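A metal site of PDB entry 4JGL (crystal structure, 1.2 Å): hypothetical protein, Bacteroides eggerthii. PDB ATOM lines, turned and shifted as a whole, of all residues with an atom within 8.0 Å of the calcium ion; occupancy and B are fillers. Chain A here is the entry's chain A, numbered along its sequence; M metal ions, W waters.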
ATOM      1  N   CYS A  35      29.550  12.992 -15.361  1.00  0.00           N
ATOM      2  CA  CYS A  35      29.436  14.404 -15.081  1.00  0.00           C
ATOM      3  C   CYS A  35      29.756  15.060 -16.385  1.00  0.00           C
ATOM      4  O   CYS A  35      30.831  14.844 -16.961  1.00  0.00           O
ATOM      5  CB  CYS A  35      30.343  14.857 -13.962  1.00  0.00           C
ATOM      6  SG  CYS A  35      29.893  16.480 -13.278  1.00  0.00           S
ATOM      7  N   ILE A 115      21.943   8.701  -3.679  1.00  0.00           N
ATOM      8  CA  ILE A 115      23.149   9.049  -2.950  1.00  0.00           C
ATOM      9  C   ILE A 115      23.787  10.298  -3.576  1.00  0.00           C
ATOM     10  O   ILE A 115      23.621  10.553  -4.766  1.00  0.00           O
ATOM     11  CB  ILE A 115      24.173   7.907  -2.916  1.00  0.00           C
ATOM     12  CG1 ILE A 115      24.731   7.592  -4.295  1.00  0.00           C
ATOM     13  CG2 ILE A 115      23.564   6.655  -2.274  1.00  0.00           C
ATOM     14  CD1 ILE A 115      25.870   6.545  -4.250  1.00  0.00           C
ATOM     15  N   PRO A 116      24.495  11.120  -2.779  1.00  0.00           N
ATOM     16  CA  PRO A 116      25.082  12.311  -3.361  1.00  0.00           C
ATOM     17  C   PRO A 116      26.121  12.020  -4.441  1.00  0.00           C
ATOM     18  O   PRO A 116      26.655  10.899  -4.524  1.00  0.00           O
ATOM     19  CB  PRO A 116      25.750  13.006  -2.167  1.00  0.00           C
ATOM     20  CG  PRO A 116      24.973  12.498  -0.994  1.00  0.00           C
ATOM     21  CD  PRO A 116      24.629  11.081  -1.317  1.00  0.00           C
ATOM     22  N   THR A 117      26.427  13.043  -5.212  1.00  0.00           N
ATOM     23  CA  THR A 117      27.469  13.019  -6.240  1.00  0.00           C
ATOM     24  C   THR A 117      28.542  14.063  -5.869  1.00  0.00           C
ATOM     25  O   THR A 117      28.568  15.156  -6.405  1.00  0.00           O
ATOM     26  CB  THR A 117      26.869  13.274  -7.620  1.00  0.00           C
ATOM     27  OG1 THR A 117      26.155  14.494  -7.601  1.00  0.00           O
ATOM     28  CG2 THR A 117      25.930  12.135  -8.018  1.00  0.00           C
ATOM     29  N   PRO A 118      29.432  13.731  -4.915  1.00  0.00           N
ATOM     30  CA  PRO A 118      30.356  14.751  -4.426  1.00  0.00           C
ATOM     31  C   PRO A 118      31.280  15.322  -5.500  1.00  0.00           C
ATOM     32  O   PRO A 118      31.719  16.471  -5.360  1.00  0.00           O
ATOM     33  CB  PRO A 118      31.157  14.016  -3.337  1.00  0.00           C
ATOM     34  CG  PRO A 118      30.939  12.563  -3.576  1.00  0.00           C
ATOM     35  CD  PRO A 118      29.598  12.434  -4.224  1.00  0.00           C
ATOM     36  N   ASP A 119      31.562  14.558  -6.538  1.00  0.00           N
ATOM     37  CA  ASP A 119      32.524  14.964  -7.557  1.00  0.00           C
ATOM     38  C   ASP A 119      31.917  15.649  -8.781  1.00  0.00           C
ATOM     39  O   ASP A 119      32.630  15.969  -9.733  1.00  0.00           O
ATOM     40  CB  ASP A 119      33.352  13.746  -7.991  1.00  0.00           C
ATOM     41  CG  ASP A 119      34.123  13.108  -6.839  1.00  0.00           C
ATOM     42  OD1 ASP A 119      34.517  13.833  -5.898  1.00  0.00           O
ATOM     43  OD2 ASP A 119      34.327  11.879  -6.882  1.00  0.00           O
ATOM     44  N   CYS A 120      30.608  15.900  -8.733  1.00  0.00           N
ATOM     45  CA  CYS A 120      29.911  16.511  -9.868  1.00  0.00           C
ATOM     46  C   CYS A 120      28.978  17.611  -9.393  1.00  0.00           C
ATOM     47  O   CYS A 120      28.014  17.350  -8.667  1.00  0.00           O
ATOM     48  CB  CYS A 120      29.092  15.463 -10.626  1.00  0.00           C
ATOM     49  SG  CYS A 120      28.226  16.148 -12.060  1.00  0.00           S
ATOM     50  N   GLU A 121      29.224  18.843  -9.821  1.00  0.00           N
ATOM     51  CA  GLU A 121      28.375  19.962  -9.402  1.00  0.00           C
ATOM     52  C   GLU A 121      27.111  20.066 -10.256  1.00  0.00           C
ATOM     53  O   GLU A 121      26.217  20.853  -9.952  1.00  0.00           O
ATOM     54  CB  GLU A 121      29.141  21.301  -9.340  1.00  0.00           C
ATOM     55  CG  GLU A 121      29.437  22.005 -10.665  1.00  0.00           C
ATOM     56  CD  GLU A 121      30.060  23.419 -10.486  1.00  0.00           C
ATOM     57  OE1 GLU A 121      30.330  23.793  -9.341  1.00  0.00           O
ATOM     58  OE2 GLU A 121      30.295  24.139 -11.485  1.00  0.00           O
ATOM     59  N   ASN A 122      27.017  19.273 -11.309  1.00  0.00           N
ATOM     60  CA  ASN A 122      25.872  19.314 -12.232  1.00  0.00           C
ATOM     61  C   ASN A 122      24.769  18.293 -11.911  1.00  0.00           C
ATOM     62  O   ASN A 122      23.789  18.176 -12.633  1.00  0.00           O
ATOM     63  CB  ASN A 122      26.350  19.099 -13.700  1.00  0.00           C
ATOM     64  CG  ASN A 122      27.139  20.242 -14.250  1.00  0.00           C
ATOM     65  OD1 ASN A 122      27.020  21.373 -13.809  1.00  0.00           O
ATOM     66  ND2 ASN A 122      27.940  19.954 -15.274  1.00  0.00           N
ATOM     67  N   SER A 123      24.940  17.561 -10.811  1.00  0.00           N
ATOM     68  CA  SER A 123      23.953  16.641 -10.319  1.00  0.00           C
ATOM     69  C   SER A 123      23.967  16.715  -8.800  1.00  0.00           C
ATOM     70  O   SER A 123      24.997  16.971  -8.160  1.00  0.00           O
ATOM     71  CB  SER A 123      24.226  15.219 -10.782  1.00  0.00           C
ATOM     72  OG  SER A 123      25.449  14.748 -10.244  1.00  0.00           O
ATOM     73  N   ALA A 124      22.805  16.451  -8.207  1.00  0.00           N
ATOM     74  CA  ALA A 124      22.652  16.410  -6.754  1.00  0.00           C
ATOM     75  C   ALA A 124      22.725  14.981  -6.199  1.00  0.00           C
ATOM     76  O   ALA A 124      23.362  14.755  -5.153  1.00  0.00           O
ATOM     77  CB  ALA A 124      21.308  17.041  -6.366  1.00  0.00           C
ATOM     78  N   TYR A 125      22.139  14.030  -6.923  1.00  0.00           N
ATOM     79  CA  TYR A 125      22.118  12.626  -6.477  1.00  0.00           C
ATOM     80  C   TYR A 125      22.152  11.709  -7.682  1.00  0.00           C
ATOM     81  O   TYR A 125      21.826  12.121  -8.809  1.00  0.00           O
ATOM     82  CB  TYR A 125      20.857  12.284  -5.662  1.00  0.00           C
ATOM     83  CG  TYR A 125      20.649  13.096  -4.430  1.00  0.00           C
ATOM     84  CD1 TYR A 125      20.039  14.332  -4.475  1.00  0.00           C
ATOM     85  CD2 TYR A 125      21.069  12.639  -3.194  1.00  0.00           C
ATOM     86  CE1 TYR A 125      19.852  15.098  -3.311  1.00  0.00           C
ATOM     87  CE2 TYR A 125      20.912  13.384  -2.059  1.00  0.00           C
ATOM     88  CZ  TYR A 125      20.307  14.612  -2.114  1.00  0.00           C
ATOM     89  OH  TYR A 125      20.148  15.375  -0.964  1.00  0.00           O
ATOM     90  N   VAL A 126      22.484  10.445  -7.437  1.00  0.00           N
ATOM     91  CA  VAL A 126      22.344   9.366  -8.401  1.00  0.00           C
ATOM     92  C   VAL A 126      21.766   8.158  -7.667  1.00  0.00           C
ATOM     93  O   VAL A 126      22.024   7.944  -6.480  1.00  0.00           O
ATOM     94  CB  VAL A 126      23.706   9.033  -9.064  1.00  0.00           C
ATOM     95  CG1 VAL A 126      24.734   8.523  -8.039  1.00  0.00           C
ATOM     96  CG2 VAL A 126      23.531   8.047 -10.245  1.00  0.00           C
ATOM     97  N   LEU A 138      19.343  12.839 -10.027  1.00  0.00           N
ATOM     98  CA  LEU A 138      18.559  14.011  -9.623  1.00  0.00           C
ATOM     99  C   LEU A 138      19.456  15.207  -9.870  1.00  0.00           C
ATOM    100  O   LEU A 138      20.468  15.394  -9.210  1.00  0.00           O
ATOM    101  CB  LEU A 138      18.167  13.952  -8.145  1.00  0.00           C
ATOM    102  CG  LEU A 138      17.290  12.793  -7.688  1.00  0.00           C
ATOM    103  CD1 LEU A 138      16.977  12.890  -6.216  1.00  0.00           C
ATOM    104  CD2 LEU A 138      16.026  12.724  -8.469  1.00  0.00           C
HETATM  105 CA    CA M   1      26.882  16.750  -6.801  1.00  0.00          CA
HETATM  106  O   HOH W   1      28.580  17.998  -5.666  1.00  0.00           O
HETATM  107  O   HOH W   2      25.995  16.024  -4.734  1.00  0.00           O
HETATM  108  O   HOH W   3      25.979  18.937  -6.412  1.00  0.00           O
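SG of Cys 120 is in hydrogen-bond range of OG of Ser 123, at 3.6 Å. The backbone NH of Asn 122 sits close to the side-chain sulfur of Cys 120. The side-chain sulfur (SG) of Cys 35 forms a disulfide with the side-chain sulfur (SG) of Cys 120 (2.1 Å).
Three residues have an atom within 4 Å of the calcium ion: Thr 117, Cys 120 and Ser 123. The nearest printed residue that does not touch the calcium ion is Ala 124 (4.2 Å).
Water W2 lies within hydrogen-bond range of the backbone carbonyl oxygen of Ala 124 and the backbone NH of Thr 117.
The calcium ion is bound by O of Cys 120, O of Ser 123, O of Thr 117, water W2, water W1, water W3 and OG1 of Thr 117. The calcium ion has seven donor atoms within binding distance.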
